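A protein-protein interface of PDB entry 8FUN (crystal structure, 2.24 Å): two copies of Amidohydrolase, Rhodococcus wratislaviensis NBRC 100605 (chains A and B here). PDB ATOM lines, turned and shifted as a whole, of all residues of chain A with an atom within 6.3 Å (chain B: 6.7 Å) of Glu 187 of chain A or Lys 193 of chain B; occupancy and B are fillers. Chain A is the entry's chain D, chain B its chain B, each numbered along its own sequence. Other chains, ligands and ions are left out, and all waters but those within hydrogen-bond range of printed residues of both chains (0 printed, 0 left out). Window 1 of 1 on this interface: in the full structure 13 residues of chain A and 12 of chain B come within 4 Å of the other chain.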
ATOM      1  N   GLU A 158       4.562 -20.949  -6.988  1.00  0.00           N
ATOM      2  CA  GLU A 158       5.208 -22.060  -7.675  1.00  0.00           C
ATOM      3  C   GLU A 158       6.149 -22.859  -6.775  1.00  0.00           C
ATOM      4  O   GLU A 158       6.653 -23.892  -7.228  1.00  0.00           O
ATOM      5  CB  GLU A 158       5.933 -21.581  -8.932  1.00  0.00           C
ATOM      6  CG  GLU A 158       5.031 -20.874  -9.954  1.00  0.00           C
ATOM      7  CD  GLU A 158       3.982 -21.780 -10.640  1.00  0.00           C
ATOM      8  OE1 GLU A 158       3.726 -22.915 -10.175  1.00  0.00           O
ATOM      9  OE2 GLU A 158       3.394 -21.340 -11.659  1.00  0.00           O
ATOM     10  N   LYS A 184      -1.354 -15.913 -14.045  1.00  0.00           N
ATOM     11  CA  LYS A 184      -0.690 -16.941 -14.834  1.00  0.00           C
ATOM     12  C   LYS A 184       0.170 -17.829 -13.947  1.00  0.00           C
ATOM     13  O   LYS A 184       0.938 -17.330 -13.112  1.00  0.00           O
ATOM     14  CB  LYS A 184       0.146 -16.311 -15.945  1.00  0.00           C
ATOM     15  CG  LYS A 184      -0.753 -15.616 -16.961  1.00  0.00           C
ATOM     16  CD  LYS A 184       0.004 -15.108 -18.143  1.00  0.00           C
ATOM     17  CE  LYS A 184      -0.948 -14.537 -19.177  1.00  0.00           C
ATOM     18  NZ  LYS A 184      -1.692 -13.341 -18.652  1.00  0.00           N
ATOM     19  N   THR A 185       0.028 -19.143 -14.127  1.00  0.00           N
ATOM     20  CA  THR A 185       0.792 -20.154 -13.407  1.00  0.00           C
ATOM     21  C   THR A 185       1.240 -21.239 -14.384  1.00  0.00           C
ATOM     22  O   THR A 185       0.748 -21.327 -15.518  1.00  0.00           O
ATOM     23  CB  THR A 185      -0.046 -20.752 -12.277  1.00  0.00           C
ATOM     24  OG1 THR A 185      -1.323 -21.139 -12.807  1.00  0.00           O
ATOM     25  CG2 THR A 185      -0.251 -19.738 -11.167  1.00  0.00           C
ATOM     26  N   LEU A 186       2.179 -22.089 -13.930  1.00  0.00           N
ATOM     27  CA  LEU A 186       2.677 -23.186 -14.766  1.00  0.00           C
ATOM     28  C   LEU A 186       1.644 -24.300 -14.927  1.00  0.00           C
ATOM     29  O   LEU A 186       1.575 -24.927 -15.987  1.00  0.00           O
ATOM     30  CB  LEU A 186       3.982 -23.744 -14.186  1.00  0.00           C
ATOM     31  CG  LEU A 186       4.745 -24.695 -15.120  1.00  0.00           C
ATOM     32  CD1 LEU A 186       5.318 -23.981 -16.350  1.00  0.00           C
ATOM     33  CD2 LEU A 186       5.859 -25.391 -14.355  1.00  0.00           C
ATOM     34  N   GLU A 187       0.845 -24.558 -13.895  1.00  0.00           N
ATOM     35  CA  GLU A 187      -0.284 -25.475 -13.890  1.00  0.00           C
ATOM     36  C   GLU A 187      -1.542 -24.693 -13.550  1.00  0.00           C
ATOM     37  O   GLU A 187      -1.463 -23.737 -12.779  1.00  0.00           O
ATOM     38  CB  GLU A 187      -0.102 -26.576 -12.837  1.00  0.00           C
ATOM     39  CG  GLU A 187       1.107 -27.431 -13.023  1.00  0.00           C
ATOM     40  CD  GLU A 187       1.216 -28.501 -11.963  1.00  0.00           C
ATOM     41  OE1 GLU A 187       0.229 -29.248 -11.778  1.00  0.00           O
ATOM     42  OE2 GLU A 187       2.292 -28.606 -11.334  1.00  0.00           O
ATOM     43  N   PRO A 188      -2.715 -25.075 -14.070  1.00  0.00           N
ATOM     44  CA  PRO A 188      -3.941 -24.363 -13.674  1.00  0.00           C
ATOM     45  C   PRO A 188      -4.156 -24.443 -12.161  1.00  0.00           C
ATOM     46  O   PRO A 188      -3.726 -25.393 -11.502  1.00  0.00           O
ATOM     47  CB  PRO A 188      -5.044 -25.087 -14.458  1.00  0.00           C
ATOM     48  CG  PRO A 188      -4.337 -25.699 -15.645  1.00  0.00           C
ATOM     49  CD  PRO A 188      -2.994 -26.115 -15.082  1.00  0.00           C
ATOM     50  N   LEU A 189      -4.808 -23.407 -11.603  1.00  0.00           N
ATOM     51  CA  LEU A 189      -4.811 -23.191 -10.148  1.00  0.00           C
ATOM     52  C   LEU A 189      -5.598 -24.231  -9.356  1.00  0.00           C
ATOM     53  O   LEU A 189      -5.413 -24.313  -8.135  1.00  0.00           O
ATOM     54  CB  LEU A 189      -5.356 -21.806  -9.778  1.00  0.00           C
ATOM     55  CG  LEU A 189      -4.368 -20.654  -9.932  1.00  0.00           C
ATOM     56  CD1 LEU A 189      -5.133 -19.324  -9.872  1.00  0.00           C
ATOM     57  CD2 LEU A 189      -3.190 -20.713  -8.932  1.00  0.00           C
ATOM     58  N   GLY A 190      -6.457 -25.014  -9.994  1.00  0.00           N
ATOM     59  CA  GLY A 190      -7.062 -26.127  -9.298  1.00  0.00           C
ATOM     60  C   GLY A 190      -6.161 -27.332  -9.126  1.00  0.00           C
ATOM     61  O   GLY A 190      -6.592 -28.312  -8.510  1.00  0.00           O
ATOM     62  N   SER A 191      -4.924 -27.287  -9.643  1.00  0.00           N
ATOM     63  CA  SER A 191      -4.019 -28.425  -9.546  1.00  0.00           C
ATOM     64  C   SER A 191      -3.640 -28.701  -8.096  1.00  0.00           C
ATOM     65  O   SER A 191      -3.504 -27.780  -7.294  1.00  0.00           O
ATOM     66  CB  SER A 191      -2.744 -28.179 -10.350  1.00  0.00           C
ATOM     67  OG  SER A 191      -1.733 -29.084  -9.922  1.00  0.00           O
ATOM     68  N   ARG A 192      -3.452 -29.990  -7.784  1.00  0.00           N
ATOM     69  CA  ARG A 192      -3.084 -30.381  -6.422  1.00  0.00           C
ATOM     70  C   ARG A 192      -1.839 -29.653  -5.946  1.00  0.00           C
ATOM     71  O   ARG A 192      -1.666 -29.438  -4.743  1.00  0.00           O
ATOM     72  CB  ARG A 192      -2.855 -31.892  -6.344  1.00  0.00           C
ATOM     73  CG  ARG A 192      -2.802 -32.416  -4.917  1.00  0.00           C
ATOM     74  CD  ARG A 192      -2.657 -33.931  -4.858  1.00  0.00           C
ATOM     75  NE  ARG A 192      -2.580 -34.376  -3.473  1.00  0.00           N
ATOM     76  CZ  ARG A 192      -3.626 -34.786  -2.762  1.00  0.00           C
ATOM     77  NH1 ARG A 192      -4.842 -34.821  -3.304  1.00  0.00           N
ATOM     78  NH2 ARG A 192      -3.448 -35.159  -1.500  1.00  0.00           N
ATOM     79  N   LYS A 193      -0.959 -29.277  -6.882  1.00  0.00           N
ATOM     80  CA  LYS A 193       0.258 -28.567  -6.513  1.00  0.00           C
ATOM     81  C   LYS A 193      -0.016 -27.426  -5.529  1.00  0.00           C
ATOM     82  O   LYS A 193       0.727 -27.252  -4.562  1.00  0.00           O
ATOM     83  CB  LYS A 193       0.960 -28.028  -7.764  1.00  0.00           C
ATOM     84  CG  LYS A 193       2.114 -27.107  -7.400  1.00  0.00           C
ATOM     85  CD  LYS A 193       2.897 -26.576  -8.601  1.00  0.00           C
ATOM     86  CE  LYS A 193       4.105 -25.771  -8.105  1.00  0.00           C
ATOM     87  NZ  LYS A 193       5.010 -25.275  -9.163  1.00  0.00           N
ATOM     88  N   TYR A 194      -1.107 -26.674  -5.735  1.00  0.00           N
ATOM     89  CA  TYR A 194      -1.356 -25.467  -4.943  1.00  0.00           C
ATOM     90  C   TYR A 194      -2.193 -25.729  -3.702  1.00  0.00           C
ATOM     91  O   TYR A 194      -2.381 -24.811  -2.888  1.00  0.00           O
ATOM     92  CB  TYR A 194      -2.025 -24.392  -5.828  1.00  0.00           C
ATOM     93  CG  TYR A 194      -1.242 -24.140  -7.123  1.00  0.00           C
ATOM     94  CD1 TYR A 194       0.041 -23.575  -7.089  1.00  0.00           C
ATOM     95  CD2 TYR A 194      -1.759 -24.513  -8.364  1.00  0.00           C
ATOM     96  CE1 TYR A 194       0.768 -23.368  -8.256  1.00  0.00           C
ATOM     97  CE2 TYR A 194      -1.036 -24.305  -9.538  1.00  0.00           C
ATOM     98  CZ  TYR A 194       0.227 -23.743  -9.479  1.00  0.00           C
ATOM     99  OH  TYR A 194       0.943 -23.527 -10.638  1.00  0.00           O
ATOM    100  N   GLY A 216       4.401 -16.765 -15.976  1.00  0.00           N
ATOM    101  CA  GLY A 216       3.721 -17.995 -15.703  1.00  0.00           C
ATOM    102  C   GLY A 216       4.398 -19.236 -16.256  1.00  0.00           C
ATOM    103  O   GLY A 216       4.271 -20.302 -15.651  1.00  0.00           O
ATOM    104  N   HIS A 218       3.991 -20.247 -19.711  1.00  0.00           N
ATOM    105  CA  HIS A 218       3.408 -20.470 -21.021  1.00  0.00           C
ATOM    106  C   HIS A 218       3.225 -19.138 -21.744  1.00  0.00           C
ATOM    107  O   HIS A 218       3.357 -18.058 -21.156  1.00  0.00           O
ATOM    108  CB  HIS A 218       2.072 -21.196 -20.875  1.00  0.00           C
ATOM    109  CG  HIS A 218       2.164 -22.405 -19.999  1.00  0.00           C
ATOM    110  ND1 HIS A 218       2.638 -23.617 -20.458  1.00  0.00           N
ATOM    111  CD2 HIS A 218       1.889 -22.579 -18.685  1.00  0.00           C
ATOM    112  CE1 HIS A 218       2.625 -24.493 -19.468  1.00  0.00           C
ATOM    113  NE2 HIS A 218       2.166 -23.892 -18.385  1.00  0.00           N
ATOM    114  N   GLN A 243      -8.336 -20.155 -15.320  1.00  0.00           N
ATOM    115  CA  GLN A 243      -8.168 -20.410 -13.895  1.00  0.00           C
ATOM    116  C   GLN A 243      -9.500 -20.687 -13.212  1.00  0.00           C
ATOM    117  O   GLN A 243      -9.562 -21.494 -12.278  1.00  0.00           O
ATOM    118  CB  GLN A 243      -7.480 -19.233 -13.204  1.00  0.00           C
ATOM    119  CG  GLN A 243      -6.062 -18.874 -13.672  1.00  0.00           C
ATOM    120  CD  GLN A 243      -5.027 -19.908 -13.307  1.00  0.00           C
ATOM    121  OE1 GLN A 243      -5.334 -21.089 -13.131  1.00  0.00           O
ATOM    122  NE2 GLN A 243      -3.807 -19.449 -13.084  1.00  0.00           N
ATOM    123  N   SER A 246     -10.549 -24.324 -14.072  1.00  0.00           N
ATOM    124  CA  SER A 246      -9.736 -25.262 -13.313  1.00  0.00           C
ATOM    125  C   SER A 246     -10.147 -25.299 -11.841  1.00  0.00           C
ATOM    126  O   SER A 246     -10.415 -26.373 -11.298  1.00  0.00           O
ATOM    127  CB  SER A 246      -8.259 -24.902 -13.462  1.00  0.00           C
ATOM    128  OG  SER A 246      -7.486 -25.596 -12.495  1.00  0.00           O
ATOM    129  N   PHE B 157       5.128 -38.708 -11.212  1.00  0.00           N
ATOM    130  CA  PHE B 157       6.091 -37.695 -10.788  1.00  0.00           C
ATOM    131  C   PHE B 157       5.480 -36.304 -10.722  1.00  0.00           C
ATOM    132  O   PHE B 157       5.958 -35.458  -9.960  1.00  0.00           O
ATOM    133  CB  PHE B 157       7.310 -37.677 -11.708  1.00  0.00           C
ATOM    134  CG  PHE B 157       8.455 -38.528 -11.203  1.00  0.00           C
ATOM    135  CD1 PHE B 157       8.472 -39.912 -11.410  1.00  0.00           C
ATOM    136  CD2 PHE B 157       9.467 -37.951 -10.444  1.00  0.00           C
ATOM    137  CE1 PHE B 157       9.512 -40.696 -10.922  1.00  0.00           C
ATOM    138  CE2 PHE B 157      10.522 -38.728  -9.937  1.00  0.00           C
ATOM    139  CZ  PHE B 157      10.545 -40.107 -10.179  1.00  0.00           C
ATOM    140  N   GLU B 158       4.441 -36.038 -11.500  1.00  0.00           N
ATOM    141  CA  GLU B 158       3.815 -34.724 -11.482  1.00  0.00           C
ATOM    142  C   GLU B 158       2.777 -34.563 -10.366  1.00  0.00           C
ATOM    143  O   GLU B 158       2.249 -33.462 -10.190  1.00  0.00           O
ATOM    144  CB  GLU B 158       3.197 -34.412 -12.861  1.00  0.00           C
ATOM    145  CG  GLU B 158       4.190 -34.536 -14.043  1.00  0.00           C
ATOM    146  CD  GLU B 158       5.329 -33.473 -14.048  1.00  0.00           C
ATOM    147  OE1 GLU B 158       5.603 -32.825 -13.011  1.00  0.00           O
ATOM    148  OE2 GLU B 158       5.972 -33.281 -15.104  1.00  0.00           O
ATOM    149  N   THR B 159       2.478 -35.618  -9.597  1.00  0.00           N
ATOM    150  CA  THR B 159       1.697 -35.492  -8.359  1.00  0.00           C
ATOM    151  C   THR B 159       2.442 -36.222  -7.247  1.00  0.00           C
ATOM    152  O   THR B 159       2.157 -37.388  -6.942  1.00  0.00           O
ATOM    153  CB  THR B 159       0.270 -36.014  -8.531  1.00  0.00           C
ATOM    154  OG1 THR B 159      -0.315 -35.408  -9.697  1.00  0.00           O
ATOM    155  CG2 THR B 159      -0.557 -35.684  -7.306  1.00  0.00           C
ATOM    156  N   PRO B 160       3.414 -35.556  -6.623  1.00  0.00           N
ATOM    157  CA  PRO B 160       4.307 -36.247  -5.677  1.00  0.00           C
ATOM    158  C   PRO B 160       3.603 -36.916  -4.506  1.00  0.00           C
ATOM    159  O   PRO B 160       4.118 -37.913  -3.979  1.00  0.00           O
ATOM    160  CB  PRO B 160       5.231 -35.113  -5.209  1.00  0.00           C
ATOM    161  CG  PRO B 160       5.295 -34.209  -6.385  1.00  0.00           C
ATOM    162  CD  PRO B 160       3.905 -34.207  -6.954  1.00  0.00           C
ATOM    163  N   LEU B 186       7.235 -31.391 -16.444  1.00  0.00           N
ATOM    164  CA  LEU B 186       6.797 -29.995 -16.601  1.00  0.00           C
ATOM    165  C   LEU B 186       7.820 -29.000 -16.054  1.00  0.00           C
ATOM    166  O   LEU B 186       7.969 -27.882 -16.581  1.00  0.00           O
ATOM    167  CB  LEU B 186       5.450 -29.775 -15.914  1.00  0.00           C
ATOM    168  CG  LEU B 186       4.733 -28.475 -16.282  1.00  0.00           C
ATOM    169  CD1 LEU B 186       4.334 -28.492 -17.723  1.00  0.00           C
ATOM    170  CD2 LEU B 186       3.509 -28.271 -15.402  1.00  0.00           C
ATOM    171  N   GLU B 187       8.513 -29.379 -14.991  1.00  0.00           N
ATOM    172  CA  GLU B 187       9.596 -28.632 -14.365  1.00  0.00           C
ATOM    173  C   GLU B 187      10.854 -29.501 -14.389  1.00  0.00           C
ATOM    174  O   GLU B 187      10.750 -30.716 -14.235  1.00  0.00           O
ATOM    175  CB  GLU B 187       9.263 -28.292 -12.908  1.00  0.00           C
ATOM    176  CG  GLU B 187       8.027 -27.451 -12.706  1.00  0.00           C
ATOM    177  CD  GLU B 187       7.735 -27.208 -11.230  1.00  0.00           C
ATOM    178  OE1 GLU B 187       8.670 -26.813 -10.506  1.00  0.00           O
ATOM    179  OE2 GLU B 187       6.571 -27.385 -10.796  1.00  0.00           O
ATOM    180  N   PRO B 188      12.043 -28.924 -14.574  1.00  0.00           N
ATOM    181  CA  PRO B 188      13.259 -29.751 -14.575  1.00  0.00           C
ATOM    182  C   PRO B 188      13.430 -30.460 -13.236  1.00  0.00           C
ATOM    183  O   PRO B 188      13.008 -29.974 -12.187  1.00  0.00           O
ATOM    184  CB  PRO B 188      14.380 -28.739 -14.835  1.00  0.00           C
ATOM    185  CG  PRO B 188      13.697 -27.599 -15.562  1.00  0.00           C
ATOM    186  CD  PRO B 188      12.343 -27.509 -14.883  1.00  0.00           C
ATOM    187  N   GLY B 190      15.549 -31.198 -10.961  1.00  0.00           N
ATOM    188  CA  GLY B 190      16.063 -30.650  -9.721  1.00  0.00           C
ATOM    189  C   GLY B 190      15.101 -29.725  -8.985  1.00  0.00           C
ATOM    190  O   GLY B 190      15.450 -29.270  -7.887  1.00  0.00           O
ATOM    191  N   SER B 191      13.920 -29.442  -9.551  1.00  0.00           N
ATOM    192  CA  SER B 191      12.938 -28.591  -8.878  1.00  0.00           C
ATOM    193  C   SER B 191      12.512 -29.213  -7.555  1.00  0.00           C
ATOM    194  O   SER B 191      12.468 -30.439  -7.408  1.00  0.00           O
ATOM    195  CB  SER B 191      11.708 -28.372  -9.770  1.00  0.00           C
ATOM    196  OG  SER B 191      10.594 -27.910  -9.022  1.00  0.00           O
ATOM    197  N   ARG B 192      12.177 -28.347  -6.588  1.00  0.00           N
ATOM    198  CA  ARG B 192      11.729 -28.802  -5.274  1.00  0.00           C
ATOM    199  C   ARG B 192      10.468 -29.652  -5.357  1.00  0.00           C
ATOM    200  O   ARG B 192      10.246 -30.506  -4.494  1.00  0.00           O
ATOM    201  CB  ARG B 192      11.466 -27.607  -4.358  1.00  0.00           C
ATOM    202  CG  ARG B 192      11.702 -27.885  -2.894  1.00  0.00           C
ATOM    203  CD  ARG B 192      11.065 -26.813  -2.019  1.00  0.00           C
ATOM    204  NE  ARG B 192      11.188 -27.119  -0.590  1.00  0.00           N
ATOM    205  CZ  ARG B 192      12.334 -27.064   0.092  1.00  0.00           C
ATOM    206  NH1 ARG B 192      12.346 -27.350   1.389  1.00  0.00           N
ATOM    207  NH2 ARG B 192      13.467 -26.727  -0.520  1.00  0.00           N
ATOM    208  N   LYS B 193       9.624 -29.420  -6.377  1.00  0.00           N
ATOM    209  CA  LYS B 193       8.409 -30.201  -6.573  1.00  0.00           C
ATOM    210  C   LYS B 193       8.644 -31.708  -6.382  1.00  0.00           C
ATOM    211  O   LYS B 193       7.820 -32.394  -5.770  1.00  0.00           O
ATOM    212  CB  LYS B 193       7.832 -29.923  -7.969  1.00  0.00           C
ATOM    213  CG  LYS B 193       6.665 -30.826  -8.346  1.00  0.00           C
ATOM    214  CD  LYS B 193       6.112 -30.577  -9.748  1.00  0.00           C
ATOM    215  CE  LYS B 193       4.931 -31.517  -9.966  1.00  0.00           C
ATOM    216  NZ  LYS B 193       4.078 -31.184 -11.130  1.00  0.00           N
ATOM    217  N   TYR B 194       9.773 -32.227  -6.878  1.00  0.00           N
ATOM    218  CA  TYR B 194      10.011 -33.669  -6.916  1.00  0.00           C
ATOM    219  C   TYR B 194      10.798 -34.175  -5.710  1.00  0.00           C
ATOM    220  O   TYR B 194      10.959 -35.393  -5.547  1.00  0.00           O
ATOM    221  CB  TYR B 194      10.746 -34.039  -8.216  1.00  0.00           C
ATOM    222  CG  TYR B 194      10.072 -33.475  -9.458  1.00  0.00           C
ATOM    223  CD1 TYR B 194       8.826 -33.952  -9.872  1.00  0.00           C
ATOM    224  CD2 TYR B 194      10.674 -32.450 -10.207  1.00  0.00           C
ATOM    225  CE1 TYR B 194       8.186 -33.435 -11.010  1.00  0.00           C
ATOM    226  CE2 TYR B 194      10.048 -31.924 -11.342  1.00  0.00           C
ATOM    227  CZ  TYR B 194       8.799 -32.420 -11.735  1.00  0.00           C
ATOM    228  OH  TYR B 194       8.190 -31.888 -12.852  1.00  0.00           O
ATOM    229  N   TRP B 195      11.289 -33.272  -4.873  1.00  0.00           N
ATOM    230  CA  TRP B 195      12.041 -33.691  -3.694  1.00  0.00           C
ATOM    231  C   TRP B 195      11.283 -34.648  -2.783  1.00  0.00           C
ATOM    232  O   TRP B 195      11.930 -35.551  -2.228  1.00  0.00           O
ATOM    233  CB  TRP B 195      12.515 -32.456  -2.916  1.00  0.00           C
ATOM    234  CG  TRP B 195      13.686 -31.770  -3.574  1.00  0.00           C
ATOM    235  CD1 TRP B 195      14.090 -31.901  -4.881  1.00  0.00           C
ATOM    236  CD2 TRP B 195      14.608 -30.864  -2.962  1.00  0.00           C
ATOM    237  NE1 TRP B 195      15.195 -31.125  -5.110  1.00  0.00           N
ATOM    238  CE2 TRP B 195      15.539 -30.482  -3.949  1.00  0.00           C
ATOM    239  CE3 TRP B 195      14.735 -30.332  -1.672  1.00  0.00           C
ATOM    240  CZ2 TRP B 195      16.587 -29.601  -3.686  1.00  0.00           C
ATOM    241  CZ3 TRP B 195      15.770 -29.460  -1.412  1.00  0.00           C
ATOM    242  CH2 TRP B 195      16.687 -29.105  -2.411  1.00  0.00           C
ATOM    243  N   PRO B 196       9.966 -34.519  -2.557  1.00  0.00           N
ATOM    244  CA  PRO B 196       9.284 -35.558  -1.766  1.00  0.00           C
ATOM    245  C   PRO B 196       9.445 -36.939  -2.362  1.00  0.00           C
ATOM    246  O   PRO B 196       9.566 -37.925  -1.620  1.00  0.00           O
ATOM    247  CB  PRO B 196       7.819 -35.098  -1.754  1.00  0.00           C
ATOM    248  CG  PRO B 196       7.903 -33.620  -1.909  1.00  0.00           C
ATOM    249  CD  PRO B 196       9.084 -33.367  -2.817  1.00  0.00           C
ATOM    250  N   ILE B 197       9.489 -37.041  -3.689  1.00  0.00           N
ATOM    251  CA  ILE B 197       9.678 -38.349  -4.297  1.00  0.00           C
ATOM    252  C   ILE B 197      11.095 -38.846  -4.042  1.00  0.00           C
ATOM    253  O   ILE B 197      11.308 -40.028  -3.732  1.00  0.00           O
ATOM    254  CB  ILE B 197       9.351 -38.294  -5.801  1.00  0.00           C
ATOM    255  CG1 ILE B 197       7.915 -37.790  -6.019  1.00  0.00           C
ATOM    256  CG2 ILE B 197       9.533 -39.677  -6.426  1.00  0.00           C
ATOM    257  CD1 ILE B 197       7.570 -37.549  -7.496  1.00  0.00           C
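The side-chain amino group (NZ) of Lys 193 of chain A is in salt-bridge range of the side-chain carboxylate (OE2) of Glu 187 of chain B (3.1 Å). The side-chain amino group (NZ) of Lys 193 of chain B is in salt-bridge range of the side-chain carboxylate (OE2) of Glu 187 of chain A, 3.1 Å away.
N of Lys 193 of chain A sits close to OG of Ser 191 of chain A, 3.1 Å away. O of Glu 187 of chain A sits at hydrogen-bond distance from OH of Tyr 194 of chain A (3.2 Å). N of Leu 186 of chain A sits at hydrogen-bond distance from O of Gly 216 of chain A (3.2 Å). The backbone NH (N) of Leu 186 of chain A lies within hydrogen-bond range of the side-chain carboxylate (OE2) of Glu 158 of chain A. The side-chain carboxylate (OE1) of Glu 187 of chain B lies within hydrogen-bond range of the side-chain hydroxyl (OG) of Ser 191 of chain B. The side-chain carboxylate of Glu 158 of chain B lies within salt-bridge range of the side-chain amino group of Lys 193 of chain B (2.9 Å).
Leu 186 of chain B touches Leu 186 of chain A. CD2 of Leu 186 of chain A touches CG of Glu 187 of chain B (3.4 Å). Leu 186 of chain B touches Glu 187 of chain A (CD2 to CG, 3.5 Å). Thr 159 of chain B touches Arg 192 of chain A.
Glu 187 of chain A touches two residues of chain B. Of the printed residues of chain B, Arg 192 of chain A touches Thr 159. Of the printed residues of chain A, Glu 187 of chain B touches Leu 186 (3.4 Å) and Lys 193 (3.1 Å). Of the printed residues of chain A, Lys 193 of chain B touches Glu 187 (3.1 Å). The nearest residue of chain A that does not touch Lys 193 of chain B is Lys 193 of chain A (5.3 Å).
Printed residues of chain A that touch a printed residue of chain B: Leu 186, Glu 187, Arg 192 and Lys 193. Of the 15 printed residues of chain B, 4 touch a printed residue of chain A. Hydrophobic or aromatic side chains of chain B that line the printed part of chain A: Leu 186. Among the printed residues, Asp or Glu carboxylates within 4 Å of a Lys or Arg side-chain nitrogen of the other chain: Glu 187 of chain A with Lys 193 of chain B and Lys 193 of chain A with Glu 187 of chain B.
Leu 186 of chain A touches its own counterpart, Leu 186 of chain B. Leu 186 of chain A touches Glu 187 of chain B, and with the chains exchanged Glu 187 of chain A touches Leu 186 of chain B. Glu 187 of chain A touches Lys 193 of chain B, and with the chains exchanged Lys 193 of chain A touches Glu 187 of chain B.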
